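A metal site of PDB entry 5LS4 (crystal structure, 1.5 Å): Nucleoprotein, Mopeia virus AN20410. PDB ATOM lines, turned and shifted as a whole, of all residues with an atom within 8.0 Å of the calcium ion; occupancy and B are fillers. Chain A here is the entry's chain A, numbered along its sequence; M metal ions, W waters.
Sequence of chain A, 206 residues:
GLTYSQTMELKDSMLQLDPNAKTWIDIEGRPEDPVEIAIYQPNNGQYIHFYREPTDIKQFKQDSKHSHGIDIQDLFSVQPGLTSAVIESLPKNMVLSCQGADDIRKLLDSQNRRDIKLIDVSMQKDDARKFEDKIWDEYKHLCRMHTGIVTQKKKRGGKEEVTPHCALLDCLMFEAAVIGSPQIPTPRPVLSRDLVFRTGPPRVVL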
ATOM      1  N   ILE A  25     -25.350 -24.340   6.807  1.00  0.00           N
ATOM      2  CA  ILE A  25     -25.542 -25.666   7.378  1.00  0.00           C
ATOM      3  C   ILE A  25     -24.208 -26.400   7.391  1.00  0.00           C
ATOM      4  O   ILE A  25     -23.399 -26.268   6.462  1.00  0.00           O
ATOM      5  CB  ILE A  25     -26.635 -26.457   6.630  1.00  0.00           C
ATOM      6  CG1 ILE A  25     -26.904 -27.802   7.295  1.00  0.00           C
ATOM      7  CG2 ILE A  25     -26.258 -26.643   5.141  1.00  0.00           C
ATOM      8  CD1 ILE A  25     -28.144 -28.504   6.773  1.00  0.00           C
ATOM      9  N   ASP A  26     -23.975 -27.155   8.470  1.00  0.00           N
ATOM     10  CA  ASP A  26     -22.764 -27.988   8.595  1.00  0.00           C
ATOM     11  C   ASP A  26     -23.145 -29.209   9.430  1.00  0.00           C
ATOM     12  O   ASP A  26     -24.001 -29.130  10.327  1.00  0.00           O
ATOM     13  CB  ASP A  26     -21.639 -27.189   9.273  1.00  0.00           C
ATOM     14  CG  ASP A  26     -20.269 -27.829   9.077  1.00  0.00           C
ATOM     15  OD1 ASP A  26     -19.598 -27.556   8.054  1.00  0.00           O
ATOM     16  OD2 ASP A  26     -19.821 -28.594   9.978  1.00  0.00           O
ATOM     17  N   ILE A  27     -22.546 -30.361   9.118  1.00  0.00           N
ATOM     18  CA  ILE A  27     -22.735 -31.589   9.885  1.00  0.00           C
ATOM     19  C   ILE A  27     -21.412 -32.233  10.255  1.00  0.00           C
ATOM     20  O   ILE A  27     -20.404 -32.098   9.548  1.00  0.00           O
ATOM     21  CB  ILE A  27     -23.669 -32.635   9.158  1.00  0.00           C
ATOM     22  CG1 ILE A  27     -22.967 -33.312   7.970  1.00  0.00           C
ATOM     23  CG2 ILE A  27     -24.956 -31.969   8.722  1.00  0.00           C
ATOM     24  CD1 ILE A  27     -23.761 -34.473   7.349  1.00  0.00           C
ATOM     25  N   GLU A  28     -21.423 -32.968  11.367  1.00  0.00           N
ATOM     26  CA  GLU A  28     -20.352 -33.901  11.661  1.00  0.00           C
ATOM     27  C   GLU A  28     -20.923 -35.311  11.657  1.00  0.00           C
ATOM     28  O   GLU A  28     -22.104 -35.524  11.999  1.00  0.00           O
ATOM     29  CB  GLU A  28     -19.661 -33.585  12.977  1.00  0.00           C
ATOM     30  CG  GLU A  28     -18.878 -32.276  12.901  1.00  0.00           C
ATOM     31  CD  GLU A  28     -17.641 -32.400  11.992  1.00  0.00           C
ATOM     32  OE1 GLU A  28     -16.991 -33.475  12.028  1.00  0.00           O
ATOM     33  OE2 GLU A  28     -17.329 -31.416  11.294  1.00  0.00           O
ATOM     34  N   GLY A  29     -20.083 -36.231  11.228  1.00  0.00           N
ATOM     35  CA  GLY A  29     -20.496 -37.605  10.942  1.00  0.00           C
ATOM     36  C   GLY A  29     -20.818 -37.785   9.465  1.00  0.00           C
ATOM     37  O   GLY A  29     -21.070 -36.828   8.750  1.00  0.00           O
ATOM     38  N   GLU A  36     -23.909 -34.587  14.613  1.00  0.00           N
ATOM     39  CA  GLU A  36     -24.041 -33.186  15.022  1.00  0.00           C
ATOM     40  C   GLU A  36     -24.453 -32.363  13.825  1.00  0.00           C
ATOM     41  O   GLU A  36     -23.876 -32.519  12.741  1.00  0.00           O
ATOM     42  CB  GLU A  36     -22.738 -32.627  15.587  1.00  0.00           C
ATOM     43  CG  GLU A  36     -22.883 -31.251  16.278  1.00  0.00           C
ATOM     44  CD  GLU A  36     -21.587 -30.661  16.764  1.00  0.00           C
ATOM     45  OE1 GLU A  36     -20.506 -30.950  16.190  1.00  0.00           O
ATOM     46  OE2 GLU A  36     -21.638 -29.915  17.762  1.00  0.00           O
ATOM     47  N   SER A  67     -11.741 -36.236  13.409  1.00  0.00           N
ATOM     48  CA  SER A  67     -12.586 -35.111  13.032  1.00  0.00           C
ATOM     49  C   SER A  67     -13.161 -34.317  14.218  1.00  0.00           C
ATOM     50  O   SER A  67     -12.742 -33.178  14.446  1.00  0.00           O
ATOM     51  CB  SER A  67     -13.708 -35.561  12.119  1.00  0.00           C
ATOM     52  OG  SER A  67     -14.389 -34.417  11.631  1.00  0.00           O
ATOM     53  N   HIS A  68     -14.116 -34.893  14.942  1.00  0.00           N
ATOM     54  CA  HIS A  68     -14.914 -34.105  15.900  1.00  0.00           C
ATOM     55  C   HIS A  68     -14.580 -34.261  17.396  1.00  0.00           C
ATOM     56  O   HIS A  68     -14.995 -33.433  18.195  1.00  0.00           O
ATOM     57  CB  HIS A  68     -16.429 -34.330  15.671  1.00  0.00           C
ATOM     58  CG  HIS A  68     -16.857 -35.758  15.717  1.00  0.00           C
ATOM     59  ND1 HIS A  68     -16.730 -36.554  16.837  1.00  0.00           N
ATOM     60  CD2 HIS A  68     -17.417 -36.536  14.764  1.00  0.00           C
ATOM     61  CE1 HIS A  68     -17.198 -37.760  16.572  1.00  0.00           C
ATOM     62  NE2 HIS A  68     -17.635 -37.776  15.319  1.00  0.00           N
ATOM     63  N   GLN A  99     -19.768 -25.234   3.313  1.00  0.00           N
ATOM     64  CA  GLN A  99     -18.399 -25.456   2.907  1.00  0.00           C
ATOM     65  C   GLN A  99     -18.234 -26.920   2.570  1.00  0.00           C
ATOM     66  O   GLN A  99     -17.975 -27.758   3.454  1.00  0.00           O
ATOM     67  CB  GLN A  99     -17.478 -24.993   4.046  1.00  0.00           C
ATOM     68  CG  GLN A  99     -16.022 -25.237   3.869  1.00  0.00           C
ATOM     69  CD  GLN A  99     -15.366 -24.407   2.773  1.00  0.00           C
ATOM     70  OE1 GLN A  99     -15.968 -23.475   2.196  1.00  0.00           O
ATOM     71  NE2 GLN A  99     -14.122 -24.737   2.492  1.00  0.00           N
ATOM     72  N   ARG A 129     -10.710 -21.736   7.684  1.00  0.00           N
ATOM     73  CA  ARG A 129     -10.474 -21.783   9.119  1.00  0.00           C
ATOM     74  C   ARG A 129      -9.564 -20.665   9.633  1.00  0.00           C
ATOM     75  O   ARG A 129      -9.001 -20.761  10.742  1.00  0.00           O
ATOM     76  CB  ARG A 129      -9.939 -23.158   9.516  1.00  0.00           C
ATOM     77  CG  ARG A 129     -10.950 -24.261   9.250  1.00  0.00           C
ATOM     78  CD  ARG A 129     -10.544 -25.635   9.756  1.00  0.00           C
ATOM     79  NE  ARG A 129     -11.629 -26.556   9.438  1.00  0.00           N
ATOM     80  CZ  ARG A 129     -12.685 -26.791  10.201  1.00  0.00           C
ATOM     81  NH1 ARG A 129     -12.811 -26.231  11.398  1.00  0.00           N
ATOM     82  NH2 ARG A 129     -13.634 -27.597   9.763  1.00  0.00           N
ATOM     83  N   PRO A 164     -10.631 -29.695  17.297  1.00  0.00           N
ATOM     84  CA  PRO A 164     -11.761 -30.522  16.848  1.00  0.00           C
ATOM     85  C   PRO A 164     -12.778 -29.739  16.024  1.00  0.00           C
ATOM     86  O   PRO A 164     -12.955 -28.533  16.207  1.00  0.00           O
ATOM     87  CB  PRO A 164     -12.383 -31.002  18.164  1.00  0.00           C
ATOM     88  CG  PRO A 164     -11.281 -30.919  19.163  1.00  0.00           C
ATOM     89  CD  PRO A 164     -10.457 -29.737  18.764  1.00  0.00           C
ATOM     90  N   HIS A 165     -13.469 -30.442  15.142  1.00  0.00           N
ATOM     91  CA  HIS A 165     -14.492 -29.835  14.311  1.00  0.00           C
ATOM     92  C   HIS A 165     -15.859 -29.947  14.958  1.00  0.00           C
ATOM     93  O   HIS A 165     -16.318 -31.042  15.283  1.00  0.00           O
ATOM     94  CB  HIS A 165     -14.503 -30.474  12.930  1.00  0.00           C
ATOM     95  CG  HIS A 165     -13.242 -30.230  12.165  1.00  0.00           C
ATOM     96  ND1 HIS A 165     -13.006 -30.782  10.923  1.00  0.00           N
ATOM     97  CD2 HIS A 165     -12.142 -29.509  12.468  1.00  0.00           C
ATOM     98  CE1 HIS A 165     -11.819 -30.404  10.497  1.00  0.00           C
ATOM     99  NE2 HIS A 165     -11.267 -29.636  11.411  1.00  0.00           N
ATOM    100  N   CYS A 166     -16.471 -28.795  15.158  1.00  0.00           N
ATOM    101  CA  CYS A 166     -17.815 -28.642  15.713  1.00  0.00           C
ATOM    102  C   CYS A 166     -18.716 -28.074  14.626  1.00  0.00           C
ATOM    103  O   CYS A 166     -18.380 -27.067  14.001  1.00  0.00           O
ATOM    104  CB  CYS A 166     -17.793 -27.699  16.921  1.00  0.00           C
ATOM    105  SG  CYS A 166     -19.394 -27.100  17.488  1.00  0.00           S
ATOM    106  N   ALA A 167     -19.865 -28.710  14.375  1.00  0.00           N
ATOM    107  CA  ALA A 167     -20.759 -28.240  13.300  1.00  0.00           C
ATOM    108  C   ALA A 167     -21.159 -26.761  13.512  1.00  0.00           C
ATOM    109  O   ALA A 167     -21.268 -25.990  12.552  1.00  0.00           O
ATOM    110  CB  ALA A 167     -21.994 -29.093  13.236  1.00  0.00           C
ATOM    111  N   LEU A 168     -21.407 -26.388  14.759  1.00  0.00           N
ATOM    112  CA  LEU A 168     -21.846 -25.021  15.070  1.00  0.00           C
ATOM    113  C   LEU A 168     -20.706 -24.025  14.886  1.00  0.00           C
ATOM    114  O   LEU A 168     -20.825 -23.058  14.131  1.00  0.00           O
ATOM    115  CB  LEU A 168     -22.421 -24.932  16.486  1.00  0.00           C
ATOM    116  CG  LEU A 168     -22.789 -23.491  16.879  1.00  0.00           C
ATOM    117  CD1 LEU A 168     -23.928 -22.930  16.020  1.00  0.00           C
ATOM    118  CD2 LEU A 168     -23.163 -23.513  18.346  1.00  0.00           C
ATOM    119  N   LEU A 169     -19.572 -24.273  15.541  1.00  0.00           N
ATOM    120  CA  LEU A 169     -18.473 -23.321  15.450  1.00  0.00           C
ATOM    121  C   LEU A 169     -17.868 -23.276  14.047  1.00  0.00           C
ATOM    122  O   LEU A 169     -17.363 -22.238  13.633  1.00  0.00           O
ATOM    123  CB  LEU A 169     -17.431 -23.592  16.539  1.00  0.00           C
ATOM    124  CG  LEU A 169     -17.678 -22.829  17.857  1.00  0.00           C
ATOM    125  CD1 LEU A 169     -19.016 -23.168  18.492  1.00  0.00           C
ATOM    126  CD2 LEU A 169     -16.528 -23.069  18.822  1.00  0.00           C
ATOM    127  N   ASP A 170     -17.969 -24.371  13.293  1.00  0.00           N
ATOM    128  CA  ASP A 170     -17.593 -24.339  11.886  1.00  0.00           C
ATOM    129  C   ASP A 170     -18.465 -23.340  11.126  1.00  0.00           C
ATOM    130  O   ASP A 170     -17.941 -22.498  10.389  1.00  0.00           O
ATOM    131  CB  ASP A 170     -17.679 -25.733  11.246  1.00  0.00           C
ATOM    132  CG  ASP A 170     -16.474 -26.601  11.550  1.00  0.00           C
ATOM    133  OD1 ASP A 170     -15.557 -26.154  12.262  1.00  0.00           O
ATOM    134  OD2 ASP A 170     -16.445 -27.751  11.035  1.00  0.00           O
ATOM    135  N   CYS A 171     -19.786 -23.376  11.315  1.00  0.00           N
ATOM    136  CA  CYS A 171     -20.645 -22.377  10.667  1.00  0.00           C
ATOM    137  C   CYS A 171     -20.212 -20.954  11.053  1.00  0.00           C
ATOM    138  O   CYS A 171     -20.126 -20.060  10.201  1.00  0.00           O
ATOM    139  CB  CYS A 171     -22.106 -22.545  11.043  1.00  0.00           C
ATOM    140  SG  CYS A 171     -22.965 -23.985  10.327  1.00  0.00           S
ATOM    141  N   PHE A 174     -16.863 -20.045   9.347  1.00  0.00           N
ATOM    142  CA  PHE A 174     -16.999 -19.898   7.909  1.00  0.00           C
ATOM    143  C   PHE A 174     -17.609 -18.538   7.615  1.00  0.00           C
ATOM    144  O   PHE A 174     -17.171 -17.841   6.679  1.00  0.00           O
ATOM    145  CB  PHE A 174     -17.838 -21.045   7.314  1.00  0.00           C
ATOM    146  CG  PHE A 174     -17.244 -22.431   7.482  1.00  0.00           C
ATOM    147  CD1 PHE A 174     -15.888 -22.617   7.699  1.00  0.00           C
ATOM    148  CD2 PHE A 174     -18.063 -23.557   7.446  1.00  0.00           C
ATOM    149  CE1 PHE A 174     -15.361 -23.891   7.873  1.00  0.00           C
ATOM    150  CE2 PHE A 174     -17.530 -24.820   7.584  1.00  0.00           C
ATOM    151  CZ  PHE A 174     -16.200 -24.998   7.804  1.00  0.00           C
HETATM  152 CA    CA M   1     -17.542 -29.407   9.969  1.00  0.00          CA
HETATM  153  O   HOH W   1     -18.225 -31.038   8.353  1.00  0.00           O
HETATM  154  O   HOH W   2     -15.415 -30.529   9.271  1.00  0.00           O
HETATM  155  O   HOH W   3     -17.145 -28.449   7.779  1.00  0.00           O
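OD1 of Asp 170 lies within salt-bridge range of NH1 of Arg 129 (2.9 Å). The side-chain carboxylate of Glu 28 sits at hydrogen-bond distance from the side-chain hydroxyl of Ser 67 (2.8 Å). O of Glu 36 sits at hydrogen-bond distance from N of Glu 28 (2.8 Å).
Ile 27 touches the calcium ion. Within 4 Å of the calcium ion: Asp 26, Ile 27, Glu 28 and Asp 170. The nearest printed residue that does not touch the calcium ion is Arg 129 (4.3 Å).
The side-chain carboxylate (OD2) of Asp 170 binds the calcium ion, at 2.3 Å. Water W1 is bound to the calcium ion, at 2.4 Å. OE2 of Glu 28 binds the calcium ion (2.4 Å). The calcium ion is bound by the side-chain carboxylate (OD2) of Asp 26 (2.4 Å). The calcium ion is bound by water W3, 2.4 Å away. Water W2 is bound to the calcium ion (2.5 Å). The calcium ion has six donor atoms within binding distance.
Water W2 bridges ND1 of His 165 (2.9 Å) and NH2 of Arg 129 (3.5 Å).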
